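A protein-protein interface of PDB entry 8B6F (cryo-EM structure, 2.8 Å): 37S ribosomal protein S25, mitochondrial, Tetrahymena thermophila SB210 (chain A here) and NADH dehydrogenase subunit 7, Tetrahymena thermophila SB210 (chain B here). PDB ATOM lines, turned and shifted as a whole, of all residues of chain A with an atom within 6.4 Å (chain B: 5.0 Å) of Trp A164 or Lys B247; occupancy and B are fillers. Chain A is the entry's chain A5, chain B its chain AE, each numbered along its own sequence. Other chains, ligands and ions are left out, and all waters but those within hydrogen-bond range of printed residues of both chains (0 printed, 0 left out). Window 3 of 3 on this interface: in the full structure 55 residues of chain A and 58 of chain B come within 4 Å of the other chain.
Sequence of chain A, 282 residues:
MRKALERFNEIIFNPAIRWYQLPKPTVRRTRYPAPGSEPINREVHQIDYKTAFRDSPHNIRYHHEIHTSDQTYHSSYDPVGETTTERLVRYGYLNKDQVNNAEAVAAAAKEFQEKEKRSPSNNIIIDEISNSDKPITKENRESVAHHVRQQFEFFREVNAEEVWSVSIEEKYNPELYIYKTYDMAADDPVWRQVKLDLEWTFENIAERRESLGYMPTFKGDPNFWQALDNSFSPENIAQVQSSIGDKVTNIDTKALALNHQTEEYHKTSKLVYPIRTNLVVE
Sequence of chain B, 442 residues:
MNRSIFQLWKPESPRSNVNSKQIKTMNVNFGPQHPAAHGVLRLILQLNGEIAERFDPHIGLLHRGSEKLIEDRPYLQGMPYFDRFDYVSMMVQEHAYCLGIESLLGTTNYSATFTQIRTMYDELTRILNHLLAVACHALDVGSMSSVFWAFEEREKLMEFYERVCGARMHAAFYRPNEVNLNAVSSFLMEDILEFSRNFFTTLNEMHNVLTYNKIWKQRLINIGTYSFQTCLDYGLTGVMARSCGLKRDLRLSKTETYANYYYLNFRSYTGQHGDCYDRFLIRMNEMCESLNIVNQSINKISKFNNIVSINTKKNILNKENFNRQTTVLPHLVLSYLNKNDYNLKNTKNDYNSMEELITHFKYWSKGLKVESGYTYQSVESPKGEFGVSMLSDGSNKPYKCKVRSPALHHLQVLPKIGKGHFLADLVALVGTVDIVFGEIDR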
ATOM      1  N   GLU A 162     -13.076  14.447 -18.689  1.00  0.00           N
ATOM      2  CA  GLU A 162     -12.875  15.511 -19.663  1.00  0.00           C
ATOM      3  C   GLU A 162     -12.555  16.829 -18.967  1.00  0.00           C
ATOM      4  O   GLU A 162     -13.042  17.116 -17.870  1.00  0.00           O
ATOM      5  CB  GLU A 162     -14.115  15.676 -20.540  1.00  0.00           C
ATOM      6  CG  GLU A 162     -14.401  14.479 -21.434  1.00  0.00           C
ATOM      7  CD  GLU A 162     -13.292  14.211 -22.433  1.00  0.00           C
ATOM      8  OE1 GLU A 162     -12.455  15.110 -22.651  1.00  0.00           O
ATOM      9  OE2 GLU A 162     -13.254  13.099 -22.999  1.00  0.00           O
ATOM     10  N   VAL A 163     -11.734  17.643 -19.629  1.00  0.00           N
ATOM     11  CA  VAL A 163     -11.234  18.883 -19.045  1.00  0.00           C
ATOM     12  C   VAL A 163     -12.042  20.075 -19.542  1.00  0.00           C
ATOM     13  O   VAL A 163     -12.249  21.045 -18.807  1.00  0.00           O
ATOM     14  CB  VAL A 163      -9.739  19.075 -19.358  1.00  0.00           C
ATOM     15  CG1 VAL A 163      -9.218  20.352 -18.722  1.00  0.00           C
ATOM     16  CG2 VAL A 163      -8.940  17.882 -18.877  1.00  0.00           C
ATOM     17  N   TRP A 164     -12.488  20.023 -20.795  1.00  0.00           N
ATOM     18  CA  TRP A 164     -13.161  21.162 -21.406  1.00  0.00           C
ATOM     19  C   TRP A 164     -14.497  20.761 -22.017  1.00  0.00           C
ATOM     20  O   TRP A 164     -15.425  21.573 -22.081  1.00  0.00           O
ATOM     21  CB  TRP A 164     -12.254  21.790 -22.469  1.00  0.00           C
ATOM     22  CG  TRP A 164     -12.928  22.818 -23.319  1.00  0.00           C
ATOM     23  CD1 TRP A 164     -12.915  24.166 -23.136  1.00  0.00           C
ATOM     24  CD2 TRP A 164     -13.711  22.578 -24.494  1.00  0.00           C
ATOM     25  NE1 TRP A 164     -13.645  24.784 -24.122  1.00  0.00           N
ATOM     26  CE2 TRP A 164     -14.144  23.829 -24.968  1.00  0.00           C
ATOM     27  CE3 TRP A 164     -14.091  21.425 -25.188  1.00  0.00           C
ATOM     28  CZ2 TRP A 164     -14.938  23.960 -26.105  1.00  0.00           C
ATOM     29  CZ3 TRP A 164     -14.878  21.557 -26.315  1.00  0.00           C
ATOM     30  CH2 TRP A 164     -15.293  22.816 -26.764  1.00  0.00           C
ATOM     31  N   SER A 165     -14.609  19.509 -22.465  1.00  0.00           N
ATOM     32  CA  SER A 165     -15.795  19.095 -23.210  1.00  0.00           C
ATOM     33  C   SER A 165     -17.058  19.203 -22.364  1.00  0.00           C
ATOM     34  O   SER A 165     -18.096  19.668 -22.848  1.00  0.00           O
ATOM     35  CB  SER A 165     -15.617  17.666 -23.721  1.00  0.00           C
ATOM     36  OG  SER A 165     -14.551  17.582 -24.650  1.00  0.00           O
ATOM     37  N   VAL A 166     -16.995  18.777 -21.105  1.00  0.00           N
ATOM     38  CA  VAL A 166     -18.162  18.748 -20.230  1.00  0.00           C
ATOM     39  C   VAL A 166     -17.771  19.309 -18.873  1.00  0.00           C
ATOM     40  O   VAL A 166     -16.680  19.032 -18.363  1.00  0.00           O
ATOM     41  CB  VAL A 166     -18.734  17.321 -20.089  1.00  0.00           C
ATOM     42  CG1 VAL A 166     -18.964  16.701 -21.458  1.00  0.00           C
ATOM     43  CG2 VAL A 166     -17.817  16.449 -19.253  1.00  0.00           C
ATOM     44  N   SER A 167     -18.663  20.104 -18.288  1.00  0.00           N
ATOM     45  CA  SER A 167     -18.423  20.673 -16.964  1.00  0.00           C
ATOM     46  C   SER A 167     -19.767  21.069 -16.368  1.00  0.00           C
ATOM     47  O   SER A 167     -20.407  22.002 -16.858  1.00  0.00           O
ATOM     48  CB  SER A 167     -17.483  21.868 -17.053  1.00  0.00           C
ATOM     49  OG  SER A 167     -17.266  22.442 -15.776  1.00  0.00           O
ATOM     50  N   GLU A 170     -19.714  24.606 -15.264  1.00  0.00           N
ATOM     51  CA  GLU A 170     -19.996  25.524 -16.361  1.00  0.00           C
ATOM     52  C   GLU A 170     -21.483  25.545 -16.682  1.00  0.00           C
ATOM     53  O   GLU A 170     -22.046  26.606 -16.979  1.00  0.00           O
ATOM     54  CB  GLU A 170     -19.185  25.127 -17.595  1.00  0.00           C
ATOM     55  CG  GLU A 170     -19.476  25.959 -18.841  1.00  0.00           C
ATOM     56  CD  GLU A 170     -19.195  27.436 -18.644  1.00  0.00           C
ATOM     57  OE1 GLU A 170     -18.547  27.792 -17.638  1.00  0.00           O
ATOM     58  OE2 GLU A 170     -19.619  28.244 -19.499  1.00  0.00           O
ATOM     59  N   LYS A 171     -22.138  24.384 -16.638  1.00  0.00           N
ATOM     60  CA  LYS A 171     -23.566  24.338 -16.931  1.00  0.00           C
ATOM     61  C   LYS A 171     -24.360  25.187 -15.946  1.00  0.00           C
ATOM     62  O   LYS A 171     -25.299  25.889 -16.338  1.00  0.00           O
ATOM     63  CB  LYS A 171     -24.058  22.890 -16.903  1.00  0.00           C
ATOM     64  CG  LYS A 171     -23.588  22.047 -18.079  1.00  0.00           C
ATOM     65  CD  LYS A 171     -24.278  22.456 -19.369  1.00  0.00           C
ATOM     66  CE  LYS A 171     -23.847  21.571 -20.527  1.00  0.00           C
ATOM     67  NZ  LYS A 171     -24.549  21.930 -21.790  1.00  0.00           N
ATOM     68  N   ARG B 242     -20.678  24.557 -33.121  1.00  0.00           N
ATOM     69  CA  ARG B 242     -20.590  25.308 -31.875  1.00  0.00           C
ATOM     70  C   ARG B 242     -21.692  26.355 -31.796  1.00  0.00           C
ATOM     71  O   ARG B 242     -22.086  26.755 -30.696  1.00  0.00           O
ATOM     72  CB  ARG B 242     -19.215  25.964 -31.757  1.00  0.00           C
ATOM     73  CG  ARG B 242     -18.121  25.007 -31.314  1.00  0.00           C
ATOM     74  CD  ARG B 242     -16.853  25.742 -30.915  1.00  0.00           C
ATOM     75  NE  ARG B 242     -16.173  26.316 -32.070  1.00  0.00           N
ATOM     76  CZ  ARG B 242     -15.259  25.683 -32.793  1.00  0.00           C
ATOM     77  NH1 ARG B 242     -14.891  24.444 -32.513  1.00  0.00           N
ATOM     78  NH2 ARG B 242     -14.696  26.310 -33.822  1.00  0.00           N
ATOM     79  N   GLY B 245     -24.294  25.249 -29.597  1.00  0.00           N
ATOM     80  CA  GLY B 245     -23.943  24.977 -28.220  1.00  0.00           C
ATOM     81  C   GLY B 245     -23.468  23.571 -27.954  1.00  0.00           C
ATOM     82  O   GLY B 245     -23.384  23.174 -26.788  1.00  0.00           O
ATOM     83  N   LEU B 246     -23.152  22.803 -28.998  1.00  0.00           N
ATOM     84  CA  LEU B 246     -22.692  21.435 -28.796  1.00  0.00           C
ATOM     85  C   LEU B 246     -21.416  21.377 -27.970  1.00  0.00           C
ATOM     86  O   LEU B 246     -21.149  20.362 -27.317  1.00  0.00           O
ATOM     87  CB  LEU B 246     -22.476  20.752 -30.142  1.00  0.00           C
ATOM     88  CG  LEU B 246     -23.739  20.237 -30.836  1.00  0.00           C
ATOM     89  CD1 LEU B 246     -23.404  19.782 -32.234  1.00  0.00           C
ATOM     90  CD2 LEU B 246     -24.397  19.108 -30.062  1.00  0.00           C
ATOM     91  N   LYS B 247     -20.623  22.444 -27.977  1.00  0.00           N
ATOM     92  CA  LYS B 247     -19.382  22.487 -27.208  1.00  0.00           C
ATOM     93  C   LYS B 247     -18.456  21.356 -27.650  1.00  0.00           C
ATOM     94  O   LYS B 247     -17.991  20.546 -26.847  1.00  0.00           O
ATOM     95  CB  LYS B 247     -19.672  22.418 -25.707  1.00  0.00           C
ATOM     96  CG  LYS B 247     -18.456  22.627 -24.827  1.00  0.00           C
ATOM     97  CD  LYS B 247     -18.841  23.198 -23.469  1.00  0.00           C
ATOM     98  CE  LYS B 247     -19.931  22.379 -22.794  1.00  0.00           C
ATOM     99  NZ  LYS B 247     -20.157  22.817 -21.388  1.00  0.00           N
ATOM    100  N   ARG B 248     -18.199  21.309 -28.954  1.00  0.00           N
ATOM    101  CA  ARG B 248     -17.385  20.271 -29.578  1.00  0.00           C
ATOM    102  C   ARG B 248     -16.179  20.935 -30.224  1.00  0.00           C
ATOM    103  O   ARG B 248     -16.308  21.590 -31.264  1.00  0.00           O
ATOM    104  CB  ARG B 248     -18.202  19.487 -30.605  1.00  0.00           C
ATOM    105  CG  ARG B 248     -17.378  18.612 -31.537  1.00  0.00           C
ATOM    106  CD  ARG B 248     -16.495  17.645 -30.770  1.00  0.00           C
ATOM    107  NE  ARG B 248     -15.786  16.743 -31.668  1.00  0.00           N
ATOM    108  CZ  ARG B 248     -14.896  15.841 -31.277  1.00  0.00           C
ATOM    109  NH1 ARG B 248     -14.572  15.697 -30.003  1.00  0.00           N
ATOM    110  NH2 ARG B 248     -14.318  15.064 -32.188  1.00  0.00           N
ATOM    111  N   ASP B 249     -15.013  20.771 -29.608  1.00  0.00           N
ATOM    112  CA  ASP B 249     -13.759  21.268 -30.155  1.00  0.00           C
ATOM    113  C   ASP B 249     -12.734  20.149 -30.080  1.00  0.00           C
ATOM    114  O   ASP B 249     -12.514  19.577 -29.009  1.00  0.00           O
ATOM    115  CB  ASP B 249     -13.270  22.501 -29.391  1.00  0.00           C
ATOM    116  CG  ASP B 249     -12.144  23.219 -30.104  1.00  0.00           C
ATOM    117  OD1 ASP B 249     -11.416  22.565 -30.877  1.00  0.00           O
ATOM    118  OD2 ASP B 249     -11.986  24.439 -29.892  1.00  0.00           O
ATOM    119  N   LEU B 252      -9.259  20.785 -27.855  1.00  0.00           N
ATOM    120  CA  LEU B 252      -9.333  20.647 -26.402  1.00  0.00           C
ATOM    121  C   LEU B 252      -9.977  19.332 -25.992  1.00  0.00           C
ATOM    122  O   LEU B 252     -10.704  19.266 -24.998  1.00  0.00           O
ATOM    123  CB  LEU B 252     -10.090  21.825 -25.798  1.00  0.00           C
ATOM    124  CG  LEU B 252      -9.421  23.192 -25.942  1.00  0.00           C
ATOM    125  CD1 LEU B 252     -10.332  24.297 -25.448  1.00  0.00           C
ATOM    126  CD2 LEU B 252      -8.106  23.214 -25.179  1.00  0.00           C
ATOM    127  N   SER B 268     -12.743  28.478 -26.056  1.00  0.00           N
ATOM    128  CA  SER B 268     -13.583  28.266 -27.223  1.00  0.00           C
ATOM    129  C   SER B 268     -14.986  28.774 -26.922  1.00  0.00           C
ATOM    130  O   SER B 268     -15.461  28.693 -25.787  1.00  0.00           O
ATOM    131  CB  SER B 268     -13.620  26.785 -27.605  1.00  0.00           C
ATOM    132  OG  SER B 268     -14.571  26.542 -28.626  1.00  0.00           O
ATOM    133  N   THR B 270     -19.208  29.362 -27.884  1.00  0.00           N
ATOM    134  CA  THR B 270     -20.411  28.777 -28.453  1.00  0.00           C
ATOM    135  C   THR B 270     -21.572  29.733 -28.224  1.00  0.00           C
ATOM    136  O   THR B 270     -21.537  30.577 -27.326  1.00  0.00           O
ATOM    137  CB  THR B 270     -20.726  27.407 -27.835  1.00  0.00           C
ATOM    138  OG1 THR B 270     -21.115  27.572 -26.466  1.00  0.00           O
ATOM    139  CG2 THR B 270     -19.513  26.492 -27.905  1.00  0.00           C
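The backbone carbonyl oxygen of Arg B248 lies within hydrogen-bond range of the guanidinium group of Arg B242.
The guanidinium group of Arg B242 is in salt-bridge range of the side-chain carboxylate of Asp B249 (3.9 Å).
Of the 8 printed residues of chain A, 3 touch a printed residue of chain B.
Hydrophobic or aromatic side chains of chain A within 4 Å of the printed part of chain B: Trp A164.
Hydrophobic or aromatic side chains of chain B within 4 Å of the printed part of chain A: Leu B252.
Among the printed residues, 7 pairs touch across the chains.
Among the printed residues, no Asp or Glu carboxylate lies within 4 Å of a Lys or Arg side-chain nitrogen of the other chain.
Trp A164 touches five residues of chain B.
Of the printed residues of chain A, Lys B247 touches Trp A164, Ser A165 and Lys A171.
Printed residues of chain A within 4 Å of Asp B249: Trp A164.
Of the printed residues of chain A, Ser B268 touches Trp A164.
Of the printed residues of chain B, Ser A165 touches Lys B247 (3.3 Å).
Leu B246 touches none of the printed residues of chain A.
The nearest printed residue of chain B that does not touch Trp A164 is Arg B242 (5.3 Å).
The nearest printed residue of chain A that does not touch Lys B247 is Glu A170 (4.1 Å).
Among the printed residues, pairs that only touch across the chains: Trp A164 with Lys B247 (3.3 Å), Trp A164 with Arg B248 (3.9 Å), Trp A164 with Asp B249 (3.3 Å), Trp A164 with Leu B252 (3.5 Å), Trp A164 with Ser B268 (3.5 Å), Ser A165 with Lys B247 (3.3 Å) and Lys A171 with Lys B247 (3.99 Å).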
